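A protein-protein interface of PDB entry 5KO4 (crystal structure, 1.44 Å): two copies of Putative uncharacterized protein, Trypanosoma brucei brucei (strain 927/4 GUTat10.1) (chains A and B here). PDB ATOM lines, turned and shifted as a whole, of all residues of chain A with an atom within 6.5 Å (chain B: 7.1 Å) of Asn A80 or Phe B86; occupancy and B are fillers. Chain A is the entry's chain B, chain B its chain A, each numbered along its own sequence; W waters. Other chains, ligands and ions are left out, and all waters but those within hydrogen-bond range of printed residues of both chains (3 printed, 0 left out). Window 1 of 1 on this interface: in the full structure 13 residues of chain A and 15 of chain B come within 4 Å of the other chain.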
ATOM      1  N   PHE A  27     -15.428 -22.635  -7.936  1.00  0.00           N
ATOM      2  CA  PHE A  27     -16.557 -22.204  -8.754  1.00  0.00           C
ATOM      3  C   PHE A  27     -17.251 -23.391  -9.418  1.00  0.00           C
ATOM      4  O   PHE A  27     -18.072 -23.186 -10.301  1.00  0.00           O
ATOM      5  CB  PHE A  27     -16.096 -21.223  -9.830  1.00  0.00           C
ATOM      6  CG  PHE A  27     -15.332 -20.039  -9.310  1.00  0.00           C
ATOM      7  CD1 PHE A  27     -15.910 -19.164  -8.408  1.00  0.00           C
ATOM      8  CD2 PHE A  27     -14.010 -19.831  -9.676  1.00  0.00           C
ATOM      9  CE1 PHE A  27     -15.176 -18.110  -7.863  1.00  0.00           C
ATOM     10  CE2 PHE A  27     -13.284 -18.753  -9.157  1.00  0.00           C
ATOM     11  CZ  PHE A  27     -13.878 -17.893  -8.268  1.00  0.00           C
ATOM     12  N   LEU A  34     -23.738 -20.676   0.450  1.00  0.00           N
ATOM     13  CA  LEU A  34     -22.750 -19.755   1.021  1.00  0.00           C
ATOM     14  C   LEU A  34     -23.468 -18.578   1.712  1.00  0.00           C
ATOM     15  O   LEU A  34     -24.630 -18.275   1.397  1.00  0.00           O
ATOM     16  CB  LEU A  34     -21.789 -19.234  -0.056  1.00  0.00           C
ATOM     17  CG  LEU A  34     -20.847 -20.259  -0.675  1.00  0.00           C
ATOM     18  CD1 LEU A  34     -20.005 -19.614  -1.763  1.00  0.00           C
ATOM     19  CD2 LEU A  34     -19.960 -20.891   0.377  1.00  0.00           C
ATOM     20  N   PRO A  35     -22.796 -17.904   2.673  1.00  0.00           N
ATOM     21  CA  PRO A  35     -23.491 -16.873   3.459  1.00  0.00           C
ATOM     22  C   PRO A  35     -24.148 -15.776   2.621  1.00  0.00           C
ATOM     23  O   PRO A  35     -23.479 -15.104   1.838  1.00  0.00           O
ATOM     24  CB  PRO A  35     -22.387 -16.292   4.336  1.00  0.00           C
ATOM     25  CG  PRO A  35     -21.382 -17.383   4.452  1.00  0.00           C
ATOM     26  CD  PRO A  35     -21.432 -18.155   3.179  1.00  0.00           C
ATOM     27  N   TYR A  37     -25.766 -15.825  -0.015  1.00  0.00           N
ATOM     28  CA  TYR A  37     -25.503 -15.903  -1.455  1.00  0.00           C
ATOM     29  C   TYR A  37     -26.731 -15.567  -2.284  1.00  0.00           C
ATOM     30  O   TYR A  37     -26.627 -14.800  -3.243  1.00  0.00           O
ATOM     31  CB  TYR A  37     -24.991 -17.294  -1.843  1.00  0.00           C
ATOM     32  CG  TYR A  37     -24.225 -17.264  -3.131  1.00  0.00           C
ATOM     33  CD1 TYR A  37     -22.879 -16.939  -3.150  1.00  0.00           C
ATOM     34  CD2 TYR A  37     -24.871 -17.434  -4.352  1.00  0.00           C
ATOM     35  CE1 TYR A  37     -22.170 -16.859  -4.338  1.00  0.00           C
ATOM     36  CE2 TYR A  37     -24.192 -17.273  -5.550  1.00  0.00           C
ATOM     37  CZ  TYR A  37     -22.833 -17.017  -5.542  1.00  0.00           C
ATOM     38  OH  TYR A  37     -22.166 -16.861  -6.723  1.00  0.00           O
ATOM     39  N   ASN A  75     -20.325 -13.179 -11.003  1.00  0.00           N
ATOM     40  CA  ASN A  75     -20.902 -13.454  -9.693  1.00  0.00           C
ATOM     41  C   ASN A  75     -19.813 -13.465  -8.649  1.00  0.00           C
ATOM     42  O   ASN A  75     -20.029 -12.968  -7.547  1.00  0.00           O
ATOM     43  CB  ASN A  75     -21.654 -14.773  -9.675  1.00  0.00           C
ATOM     44  CG  ASN A  75     -22.973 -14.724 -10.390  1.00  0.00           C
ATOM     45  OD1 ASN A  75     -23.492 -13.651 -10.715  1.00  0.00           O
ATOM     46  ND2 ASN A  75     -23.520 -15.887 -10.688  1.00  0.00           N
ATOM     47  N   CYS A  76     -18.614 -13.955  -8.994  1.00  0.00           N
ATOM     48  CA  CYS A  76     -17.522 -13.917  -8.045  1.00  0.00           C
ATOM     49  C   CYS A  76     -17.212 -12.484  -7.639  1.00  0.00           C
ATOM     50  O   CYS A  76     -17.042 -12.213  -6.450  1.00  0.00           O
ATOM     51  CB  CYS A  76     -16.290 -14.594  -8.618  1.00  0.00           C
ATOM     52  SG  CYS A  76     -14.863 -14.559  -7.513  1.00  0.00           S
ATOM     53  N   TYR A  77     -17.161 -11.558  -8.602  1.00  0.00           N
ATOM     54  CA  TYR A  77     -16.811 -10.173  -8.279  1.00  0.00           C
ATOM     55  C   TYR A  77     -17.916  -9.492  -7.492  1.00  0.00           C
ATOM     56  O   TYR A  77     -17.631  -8.609  -6.687  1.00  0.00           O
ATOM     57  CB  TYR A  77     -16.507  -9.355  -9.550  1.00  0.00           C
ATOM     58  CG  TYR A  77     -15.510  -9.996 -10.493  1.00  0.00           C
ATOM     59  CD1 TYR A  77     -14.388 -10.653 -10.008  1.00  0.00           C
ATOM     60  CD2 TYR A  77     -15.708  -9.973 -11.867  1.00  0.00           C
ATOM     61  CE1 TYR A  77     -13.501 -11.292 -10.864  1.00  0.00           C
ATOM     62  CE2 TYR A  77     -14.825 -10.598 -12.732  1.00  0.00           C
ATOM     63  CZ  TYR A  77     -13.724 -11.263 -12.223  1.00  0.00           C
ATOM     64  OH  TYR A  77     -12.843 -11.908 -13.065  1.00  0.00           O
ATOM     65  N   ASP A  78     -19.165  -9.871  -7.726  1.00  0.00           N
ATOM     66  CA  ASP A  78     -20.282  -9.259  -7.008  1.00  0.00           C
ATOM     67  C   ASP A  78     -20.390  -9.796  -5.584  1.00  0.00           C
ATOM     68  O   ASP A  78     -20.893  -9.096  -4.721  1.00  0.00           O
ATOM     69  CB  ASP A  78     -21.591  -9.518  -7.759  1.00  0.00           C
ATOM     70  CG  ASP A  78     -21.695  -8.805  -9.087  1.00  0.00           C
ATOM     71  OD1 ASP A  78     -20.851  -7.921  -9.358  1.00  0.00           O
ATOM     72  OD2 ASP A  78     -22.621  -9.126  -9.858  1.00  0.00           O
ATOM     73  N   TYR A  79     -19.962 -11.041  -5.351  1.00  0.00           N
ATOM     74  CA  TYR A  79     -20.053 -11.678  -4.039  1.00  0.00           C
ATOM     75  C   TYR A  79     -18.798 -11.420  -3.202  1.00  0.00           C
ATOM     76  O   TYR A  79     -18.907 -10.987  -2.056  1.00  0.00           O
ATOM     77  CB  TYR A  79     -20.271 -13.180  -4.189  1.00  0.00           C
ATOM     78  CG  TYR A  79     -20.502 -13.883  -2.869  1.00  0.00           C
ATOM     79  CD1 TYR A  79     -21.695 -13.729  -2.175  1.00  0.00           C
ATOM     80  CD2 TYR A  79     -19.530 -14.711  -2.319  1.00  0.00           C
ATOM     81  CE1 TYR A  79     -21.910 -14.372  -0.965  1.00  0.00           C
ATOM     82  CE2 TYR A  79     -19.746 -15.380  -1.122  1.00  0.00           C
ATOM     83  CZ  TYR A  79     -20.942 -15.221  -0.453  1.00  0.00           C
ATOM     84  OH  TYR A  79     -21.121 -15.845   0.762  1.00  0.00           O
ATOM     85  N   ASN A  80     -17.632 -11.714  -3.749  1.00  0.00           N
ATOM     86  CA  ASN A  80     -16.361 -11.564  -3.049  1.00  0.00           C
ATOM     87  C   ASN A  80     -15.760 -10.194  -3.247  1.00  0.00           C
ATOM     88  O   ASN A  80     -15.999  -9.512  -4.254  1.00  0.00           O
ATOM     89  CB  ASN A  80     -15.366 -12.615  -3.530  1.00  0.00           C
ATOM     90  CG  ASN A  80     -15.841 -14.016  -3.310  1.00  0.00           C
ATOM     91  OD1 ASN A  80     -15.909 -14.486  -2.191  1.00  0.00           O
ATOM     92  ND2 ASN A  80     -16.331 -14.669  -4.352  1.00  0.00           N
ATOM     93  N   ARG A  81     -14.899  -9.812  -2.324  1.00  0.00           N
ATOM     94  CA  ARG A  81     -14.218  -8.539  -2.417  1.00  0.00           C
ATOM     95  C   ARG A  81     -13.136  -8.574  -3.517  1.00  0.00           C
ATOM     96  O   ARG A  81     -12.593  -9.644  -3.822  1.00  0.00           O
ATOM     97  CB  ARG A  81     -13.600  -8.180  -1.059  1.00  0.00           C
ATOM     98  CG  ARG A  81     -14.638  -7.685  -0.054  1.00  0.00           C
ATOM     99  CD  ARG A  81     -15.007  -6.222  -0.283  1.00  0.00           C
ATOM    100  NE  ARG A  81     -13.838  -5.363  -0.160  1.00  0.00           N
ATOM    101  CZ  ARG A  81     -13.299  -4.952   0.990  1.00  0.00           C
ATOM    102  NH1 ARG A  81     -13.878  -5.252   2.155  1.00  0.00           N
ATOM    103  NH2 ARG A  81     -12.190  -4.226   0.986  1.00  0.00           N
ATOM    104  N   GLU A  82     -12.802  -7.403  -4.081  1.00  0.00           N
ATOM    105  CA  GLU A  82     -11.778  -7.285  -5.129  1.00  0.00           C
ATOM    106  C   GLU A  82     -10.436  -7.834  -4.645  1.00  0.00           C
ATOM    107  O   GLU A  82      -9.741  -8.509  -5.398  1.00  0.00           O
ATOM    108  CB  GLU A  82     -11.627  -5.802  -5.552  1.00  0.00           C
ATOM    109  CG  GLU A  82     -10.781  -5.561  -6.793  1.00  0.00           C
ATOM    110  CD  GLU A  82      -9.284  -5.474  -6.560  1.00  0.00           C
ATOM    111  OE1 GLU A  82      -8.858  -4.664  -5.705  1.00  0.00           O
ATOM    112  OE2 GLU A  82      -8.532  -6.186  -7.264  1.00  0.00           O
ATOM    113  N   GLU A  83     -10.114  -7.616  -3.375  1.00  0.00           N
ATOM    114  CA  GLU A  83      -8.833  -8.032  -2.799  1.00  0.00           C
ATOM    115  C   GLU A  83      -8.776  -9.517  -2.456  1.00  0.00           C
ATOM    116  O   GLU A  83      -7.703 -10.015  -2.133  1.00  0.00           O
ATOM    117  CB  GLU A  83      -8.559  -7.218  -1.527  1.00  0.00           C
ATOM    118  CG  GLU A  83      -8.609  -5.703  -1.734  1.00  0.00           C
ATOM    119  CD  GLU A  83      -9.964  -5.040  -1.529  1.00  0.00           C
ATOM    120  OE1 GLU A  83     -10.998  -5.744  -1.640  1.00  0.00           O
ATOM    121  OE2 GLU A  83      -9.997  -3.807  -1.320  1.00  0.00           O
ATOM    122  N   SER A  84      -9.922 -10.237  -2.527  1.00  0.00           N
ATOM    123  CA  SER A  84      -9.952 -11.654  -2.199  1.00  0.00           C
ATOM    124  C   SER A  84      -9.184 -12.458  -3.208  1.00  0.00           C
ATOM    125  O   SER A  84      -9.401 -12.280  -4.414  1.00  0.00           O
ATOM    126  CB  SER A  84     -11.384 -12.183  -2.179  1.00  0.00           C
ATOM    127  OG  SER A  84     -11.396 -13.597  -2.011  1.00  0.00           O
ATOM    128  N   PHE A  86     -10.111 -15.228  -4.178  1.00  0.00           N
ATOM    129  CA  PHE A  86     -11.126 -15.821  -5.052  1.00  0.00           C
ATOM    130  C   PHE A  86     -11.272 -14.957  -6.310  1.00  0.00           C
ATOM    131  O   PHE A  86     -11.364 -15.483  -7.417  1.00  0.00           O
ATOM    132  CB  PHE A  86     -12.481 -15.890  -4.351  1.00  0.00           C
ATOM    133  CG  PHE A  86     -12.677 -17.007  -3.352  1.00  0.00           C
ATOM    134  CD1 PHE A  86     -11.590 -17.705  -2.836  1.00  0.00           C
ATOM    135  CD2 PHE A  86     -13.947 -17.460  -3.043  1.00  0.00           C
ATOM    136  CE1 PHE A  86     -11.780 -18.763  -1.945  1.00  0.00           C
ATOM    137  CE2 PHE A  86     -14.132 -18.538  -2.176  1.00  0.00           C
ATOM    138  CZ  PHE A  86     -13.045 -19.174  -1.626  1.00  0.00           C
ATOM    139  N   SER A  87     -11.332 -13.631  -6.130  1.00  0.00           N
ATOM    140  CA  SER A  87     -11.434 -12.695  -7.250  1.00  0.00           C
ATOM    141  C   SER A  87     -10.152 -12.669  -8.066  1.00  0.00           C
ATOM    142  O   SER A  87     -10.234 -12.554  -9.288  1.00  0.00           O
ATOM    143  CB  SER A  87     -11.765 -11.297  -6.756  1.00  0.00           C
ATOM    144  OG  SER A  87     -13.094 -11.310  -6.266  1.00  0.00           O
ATOM    145  N   ILE B  26     -18.626 -23.957   6.681  1.00  0.00           N
ATOM    146  CA  ILE B  26     -17.737 -23.075   5.911  1.00  0.00           C
ATOM    147  C   ILE B  26     -16.350 -23.007   6.563  1.00  0.00           C
ATOM    148  O   ILE B  26     -15.330 -22.980   5.865  1.00  0.00           O
ATOM    149  CB  ILE B  26     -18.367 -21.632   5.832  1.00  0.00           C
ATOM    150  CG1 ILE B  26     -19.778 -21.650   5.145  1.00  0.00           C
ATOM    151  CG2 ILE B  26     -17.448 -20.686   5.095  1.00  0.00           C
ATOM    152  CD1 ILE B  26     -19.825 -22.321   3.800  1.00  0.00           C
ATOM    153  N   PHE B  27     -16.303 -22.982   7.900  1.00  0.00           N
ATOM    154  CA  PHE B  27     -15.041 -22.875   8.619  1.00  0.00           C
ATOM    155  C   PHE B  27     -14.707 -24.158   9.399  1.00  0.00           C
ATOM    156  O   PHE B  27     -13.851 -24.126  10.287  1.00  0.00           O
ATOM    157  CB  PHE B  27     -15.113 -21.691   9.592  1.00  0.00           C
ATOM    158  CG  PHE B  27     -15.542 -20.406   8.934  1.00  0.00           C
ATOM    159  CD1 PHE B  27     -14.749 -19.805   7.974  1.00  0.00           C
ATOM    160  CD2 PHE B  27     -16.776 -19.839   9.215  1.00  0.00           C
ATOM    161  CE1 PHE B  27     -15.150 -18.641   7.348  1.00  0.00           C
ATOM    162  CE2 PHE B  27     -17.182 -18.667   8.579  1.00  0.00           C
ATOM    163  CZ  PHE B  27     -16.363 -18.072   7.656  1.00  0.00           C
ATOM    164  N   CYS B  76     -10.642 -15.584   8.604  1.00  0.00           N
ATOM    165  CA  CYS B  76     -11.676 -15.266   7.628  1.00  0.00           C
ATOM    166  C   CYS B  76     -11.599 -13.795   7.240  1.00  0.00           C
ATOM    167  O   CYS B  76     -11.649 -13.465   6.053  1.00  0.00           O
ATOM    168  CB  CYS B  76     -13.049 -15.611   8.173  1.00  0.00           C
ATOM    169  SG  CYS B  76     -14.412 -15.146   7.076  1.00  0.00           S
ATOM    170  N   TYR B  77     -11.472 -12.910   8.224  1.00  0.00           N
ATOM    171  CA  TYR B  77     -11.419 -11.488   7.908  1.00  0.00           C
ATOM    172  C   TYR B  77     -10.203 -11.175   7.080  1.00  0.00           C
ATOM    173  O   TYR B  77     -10.289 -10.378   6.147  1.00  0.00           O
ATOM    174  CB  TYR B  77     -11.435 -10.618   9.172  1.00  0.00           C
ATOM    175  CG  TYR B  77     -12.531 -10.939  10.176  1.00  0.00           C
ATOM    176  CD1 TYR B  77     -13.744 -11.484   9.768  1.00  0.00           C
ATOM    177  CD2 TYR B  77     -12.307 -10.807  11.540  1.00  0.00           C
ATOM    178  CE1 TYR B  77     -14.720 -11.858  10.698  1.00  0.00           C
ATOM    179  CE2 TYR B  77     -13.272 -11.181  12.473  1.00  0.00           C
ATOM    180  CZ  TYR B  77     -14.461 -11.742  12.046  1.00  0.00           C
ATOM    181  OH  TYR B  77     -15.416 -12.138  12.956  1.00  0.00           O
ATOM    182  N   TYR B  79      -8.443 -13.193   5.010  1.00  0.00           N
ATOM    183  CA  TYR B  79      -8.458 -13.791   3.683  1.00  0.00           C
ATOM    184  C   TYR B  79      -9.544 -13.164   2.793  1.00  0.00           C
ATOM    185  O   TYR B  79      -9.288 -12.820   1.637  1.00  0.00           O
ATOM    186  CB  TYR B  79      -8.684 -15.306   3.811  1.00  0.00           C
ATOM    187  CG  TYR B  79      -8.640 -16.041   2.493  1.00  0.00           C
ATOM    188  CD1 TYR B  79      -7.430 -16.350   1.890  1.00  0.00           C
ATOM    189  CD2 TYR B  79      -9.806 -16.486   1.884  1.00  0.00           C
ATOM    190  CE1 TYR B  79      -7.380 -17.072   0.703  1.00  0.00           C
ATOM    191  CE2 TYR B  79      -9.775 -17.149   0.669  1.00  0.00           C
ATOM    192  CZ  TYR B  79      -8.560 -17.471   0.091  1.00  0.00           C
ATOM    193  OH  TYR B  79      -8.568 -18.153  -1.101  1.00  0.00           O
ATOM    194  N   ASN B  80     -10.764 -13.041   3.318  1.00  0.00           N
ATOM    195  CA  ASN B  80     -11.901 -12.543   2.536  1.00  0.00           C
ATOM    196  C   ASN B  80     -12.109 -11.033   2.633  1.00  0.00           C
ATOM    197  O   ASN B  80     -12.933 -10.483   1.898  1.00  0.00           O
ATOM    198  CB  ASN B  80     -13.159 -13.228   3.021  1.00  0.00           C
ATOM    199  CG  ASN B  80     -13.084 -14.726   2.852  1.00  0.00           C
ATOM    200  OD1 ASN B  80     -13.091 -15.226   1.734  1.00  0.00           O
ATOM    201  ND2 ASN B  80     -12.948 -15.476   3.959  1.00  0.00           N
ATOM    202  N   ARG B  81     -11.364 -10.375   3.539  1.00  0.00           N
ATOM    203  CA  ARG B  81     -11.509  -8.966   3.933  1.00  0.00           C
ATOM    204  C   ARG B  81     -12.614  -8.863   4.962  1.00  0.00           C
ATOM    205  O   ARG B  81     -13.520  -9.705   5.019  1.00  0.00           O
ATOM    206  CB  ARG B  81     -11.744  -7.999   2.766  1.00  0.00           C
ATOM    207  CG  ARG B  81     -10.690  -8.096   1.654  1.00  0.00           C
ATOM    208  CD  ARG B  81      -9.257  -7.804   2.099  1.00  0.00           C
ATOM    209  NE  ARG B  81      -9.097  -6.390   2.439  1.00  0.00           N
ATOM    210  CZ  ARG B  81      -7.951  -5.718   2.425  1.00  0.00           C
ATOM    211  NH1 ARG B  81      -6.820  -6.323   2.073  1.00  0.00           N
ATOM    212  NH2 ARG B  81      -7.929  -4.427   2.736  1.00  0.00           N
ATOM    213  N   GLU B  82     -12.529  -7.840   5.798  1.00  0.00           N
ATOM    214  CA  GLU B  82     -13.414  -7.657   6.947  1.00  0.00           C
ATOM    215  C   GLU B  82     -14.834  -7.468   6.533  1.00  0.00           C
ATOM    216  O   GLU B  82     -15.724  -8.083   7.115  1.00  0.00           O
ATOM    217  CB  GLU B  82     -12.972  -6.445   7.763  1.00  0.00           C
ATOM    218  CG  GLU B  82     -11.572  -6.562   8.352  1.00  0.00           C
ATOM    219  CD  GLU B  82     -11.473  -7.005   9.795  1.00  0.00           C
ATOM    220  OE1 GLU B  82     -12.497  -6.969  10.523  1.00  0.00           O
ATOM    221  OE2 GLU B  82     -10.345  -7.348  10.215  1.00  0.00           O
ATOM    222  N   GLU B  83     -15.075  -6.571   5.569  1.00  0.00           N
ATOM    223  CA  GLU B  83     -16.418  -6.329   5.062  1.00  0.00           C
ATOM    224  C   GLU B  83     -16.616  -7.192   3.839  1.00  0.00           C
ATOM    225  O   GLU B  83     -16.201  -6.827   2.733  1.00  0.00           O
ATOM    226  CB  GLU B  83     -16.630  -4.862   4.729  1.00  0.00           C
ATOM    227  CG  GLU B  83     -16.632  -3.963   5.946  1.00  0.00           C
ATOM    228  CD  GLU B  83     -17.136  -2.573   5.621  1.00  0.00           C
ATOM    229  OE1 GLU B  83     -16.365  -1.785   5.028  1.00  0.00           O
ATOM    230  OE2 GLU B  83     -18.346  -2.323   5.825  1.00  0.00           O
ATOM    231  N   SER B  84     -17.186  -8.375   4.041  1.00  0.00           N
ATOM    232  CA  SER B  84     -17.456  -9.311   2.953  1.00  0.00           C
ATOM    233  C   SER B  84     -18.519 -10.306   3.390  1.00  0.00           C
ATOM    234  O   SER B  84     -18.683 -10.531   4.587  1.00  0.00           O
ATOM    235  CB  SER B  84     -16.190 -10.060   2.570  1.00  0.00           C
ATOM    236  OG  SER B  84     -15.827 -11.000   3.568  1.00  0.00           O
ATOM    237  N   PRO B  85     -19.204 -10.984   2.456  1.00  0.00           N
ATOM    238  CA  PRO B  85     -20.241 -11.938   2.875  1.00  0.00           C
ATOM    239  C   PRO B  85     -19.696 -13.114   3.712  1.00  0.00           C
ATOM    240  O   PRO B  85     -20.324 -13.505   4.691  1.00  0.00           O
ATOM    241  CB  PRO B  85     -20.824 -12.409   1.547  1.00  0.00           C
ATOM    242  CG  PRO B  85     -20.638 -11.265   0.648  1.00  0.00           C
ATOM    243  CD  PRO B  85     -19.274 -10.737   1.006  1.00  0.00           C
ATOM    244  N   PHE B  86     -18.504 -13.653   3.390  1.00  0.00           N
ATOM    245  CA  PHE B  86     -17.966 -14.705   4.253  1.00  0.00           C
ATOM    246  C   PHE B  86     -17.757 -14.175   5.685  1.00  0.00           C
ATOM    247  O   PHE B  86     -18.051 -14.857   6.675  1.00  0.00           O
ATOM    248  CB  PHE B  86     -16.633 -15.227   3.716  1.00  0.00           C
ATOM    249  CG  PHE B  86     -16.760 -16.249   2.615  1.00  0.00           C
ATOM    250  CD1 PHE B  86     -17.241 -17.515   2.879  1.00  0.00           C
ATOM    251  CD2 PHE B  86     -16.379 -15.947   1.314  1.00  0.00           C
ATOM    252  CE1 PHE B  86     -17.326 -18.471   1.867  1.00  0.00           C
ATOM    253  CE2 PHE B  86     -16.461 -16.904   0.309  1.00  0.00           C
ATOM    254  CZ  PHE B  86     -16.958 -18.149   0.586  1.00  0.00           C
ATOM    255  N   SER B  87     -17.223 -12.953   5.793  1.00  0.00           N
ATOM    256  CA  SER B  87     -16.943 -12.360   7.082  1.00  0.00           C
ATOM    257  C   SER B  87     -18.230 -12.029   7.859  1.00  0.00           C
ATOM    258  O   SER B  87     -18.183 -11.997   9.070  1.00  0.00           O
ATOM    259  CB  SER B  87     -16.082 -11.133   6.920  1.00  0.00           C
ATOM    260  OG  SER B  87     -14.810 -11.576   6.474  1.00  0.00           O
ATOM    261  N   THR B  88     -19.381 -11.805   7.176  1.00  0.00           N
ATOM    262  CA  THR B  88     -20.627 -11.566   7.930  1.00  0.00           C
ATOM    263  C   THR B  88     -20.967 -12.783   8.771  1.00  0.00           C
ATOM    264  O   THR B  88     -21.356 -12.619   9.922  1.00  0.00           O
ATOM    265  CB  THR B  88     -21.834 -11.170   7.046  1.00  0.00           C
ATOM    266  OG1 THR B  88     -22.205 -12.250   6.171  1.00  0.00           O
ATOM    267  CG2 THR B  88     -21.580  -9.934   6.245  1.00  0.00           C
ATOM    268  N   LEU B  89     -20.813 -13.995   8.226  1.00  0.00           N
ATOM    269  CA  LEU B  89     -21.101 -15.213   9.008  1.00  0.00           C
ATOM    270  C   LEU B  89     -20.058 -15.363  10.137  1.00  0.00           C
ATOM    271  O   LEU B  89     -20.418 -15.602  11.293  1.00  0.00           O
ATOM    272  CB  LEU B  89     -21.077 -16.461   8.127  1.00  0.00           C
ATOM    273  CG  LEU B  89     -21.215 -17.788   8.893  1.00  0.00           C
ATOM    274  CD1 LEU B  89     -22.527 -17.831   9.719  1.00  0.00           C
ATOM    275  CD2 LEU B  89     -21.105 -18.973   7.948  1.00  0.00           C
ATOM    276  N   ALA B  90     -18.777 -15.183   9.823  1.00  0.00           N
ATOM    277  CA  ALA B  90     -17.747 -15.288  10.857  1.00  0.00           C
ATOM    278  C   ALA B  90     -17.987 -14.271  11.975  1.00  0.00           C
ATOM    279  O   ALA B  90     -17.782 -14.598  13.137  1.00  0.00           O
ATOM    280  CB  ALA B  90     -16.365 -15.078  10.258  1.00  0.00           C
ATOM    281  N   ARG B  91     -18.472 -13.058  11.638  1.00  0.00           N
ATOM    282  CA  ARG B  91     -18.749 -12.043  12.662  1.00  0.00           C
ATOM    283  C   ARG B  91     -19.889 -12.485  13.567  1.00  0.00           C
ATOM    284  O   ARG B  91     -19.802 -12.286  14.779  1.00  0.00           O
ATOM    285  CB  ARG B  91     -19.097 -10.690  12.025  1.00  0.00           C
ATOM    286  CG  ARG B  91     -17.881  -9.921  11.492  1.00  0.00           C
ATOM    287  CD  ARG B  91     -17.022  -9.378  12.570  1.00  0.00           C
ATOM    288  NE  ARG B  91     -16.638  -7.981  12.355  1.00  0.00           N
ATOM    289  CZ  ARG B  91     -15.593  -7.571  11.640  1.00  0.00           C
ATOM    290  NH1 ARG B  91     -14.887  -8.435  10.921  1.00  0.00           N
ATOM    291  NH2 ARG B  91     -15.281  -6.289  11.592  1.00  0.00           N
HETATM  292  O   HOH W   1     -13.661 -14.053  -0.635  1.00  0.00           O
HETATM  293  O   HOH W   2     -17.012 -12.903   0.659  1.00  0.00           O
HETATM  294  O   HOH W   3     -14.555 -11.558  -0.042  1.00  0.00           O
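The guanidinium group (NH1) of Arg A81 sits at hydrogen-bond distance from the backbone carbonyl oxygen (O) of Glu B83, 2.9 Å away.
The side-chain sulfur (SG) of Cys B76 lies within hydrogen-bond range of the backbone carbonyl oxygen (O) of Phe B86, at 3.7 Å. O of Arg B81 lies within hydrogen-bond range of OG of Ser B84 (3.0 Å). The side-chain hydroxyl (OG) of Ser B87 is in hydrogen-bond range of the backbone carbonyl oxygen (O) of Arg B81, 2.7 Å away. The backbone carbonyl oxygen (O) of Cys A76 is in hydrogen-bond range of the side-chain amide nitrogen (ND2) of Asn A80. The side-chain sulfur (SG) of Cys A76 is in hydrogen-bond range of the backbone carbonyl oxygen (O) of Phe A86. The guanidinium group of Arg A81 is in salt-bridge range of the side-chain carboxylate of Glu A83.
Among the printed residues, merely in contact across the chains: Leu A34 with Ile B26 (3.7 Å), Leu A34 with Phe B86 (3.9 Å), Pro A35 with Pro B85 (3.5 Å), Pro A35 with Leu B89 (3.8 Å), Tyr A79 with Pro B85 (3.1 Å), Tyr A79 with Phe B86 (3.9 Å), Asn A80 with Phe B86 (3.5 Å), Arg A81 with Asn B80 (3.8 Å), Arg A81 with Arg B81 (3.5 Å), Arg A81 with Ser B84 (3.9 Å), Glu A83 with Arg B81 (3.7 Å), Phe A86 with Tyr B79 (3.4 Å) and Phe A86 with Phe B86 (3.8 Å).
Asn A75 touches none of the printed residues of chain B. Asn A80 touches just one residue of chain B: Phe B86. Of the printed residues of chain B, Glu A83 touches Arg B81 (3.7 Å). Printed residues of chain B within 4 Å of Phe A86: Tyr B79 (3.4 Å) and Phe B86 (3.8 Å). Phe B27 touches none of the printed residues of chain A. Printed residues of chain A within 4 Å of Asn B80: Arg A81. Printed residues of chain A within 4 Å of Phe B86: Leu A34, Tyr A79, Asn A80 and Phe A86. Of the printed residues of chain A, Leu B89 touches Pro A35 (3.8 Å). The nearest residue of chain B that does not touch Asn A80 is Asn B80 (4.9 Å). The nearest residue of chain A that does not touch Phe B86 is Pro A35 (4.3 Å). The nearest printed residue of chain A that does not touch Arg B81 is Ser A84 (4.8 Å).
Hydrophobic or aromatic side chains of chain A within 4 Å of the printed part of chain B: Leu A34, Pro A35, Tyr A79 and Phe A86. Hydrophobic or aromatic side chains of chain B that line the printed part of chain A: Ile B26, Tyr B79, Pro B85, Phe B86 and Leu B89. Among the printed residues, no Asp or Glu carboxylate lies within 4 Å of a Lys or Arg side-chain nitrogen of the other chain.
Tyr A79 touches Phe B86, and with the chains exchanged Phe A86 touches Tyr B79. Arg A81 touches its own counterpart, Arg B81. Arg A81 touches Glu B83, and with the chains exchanged Glu A83 touches Arg B81. Phe B86 touches its own counterpart, Phe A86. Positions printed for both chains: 27, 76, 77, 79, 80, 81, 82, 83, 84, 86 and 87. Of the 14 pairs that touch across the chains among the printed residues, 6 have their exchanged pair printed and touching as well.
Water W1 lies within hydrogen-bond range of OG of Ser A84 (2.7 Å), OD1 of Asn B80 (2.7 Å) and OD1 of Asn A80 (2.8 Å). Water W3 lies within hydrogen-bond range of the backbone carbonyl oxygen (O) of Asn B80 and the backbone NH (N) of Arg A81. Water W2 lies within hydrogen-bond range of N of Phe B86 and OD1 of Asn A80.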
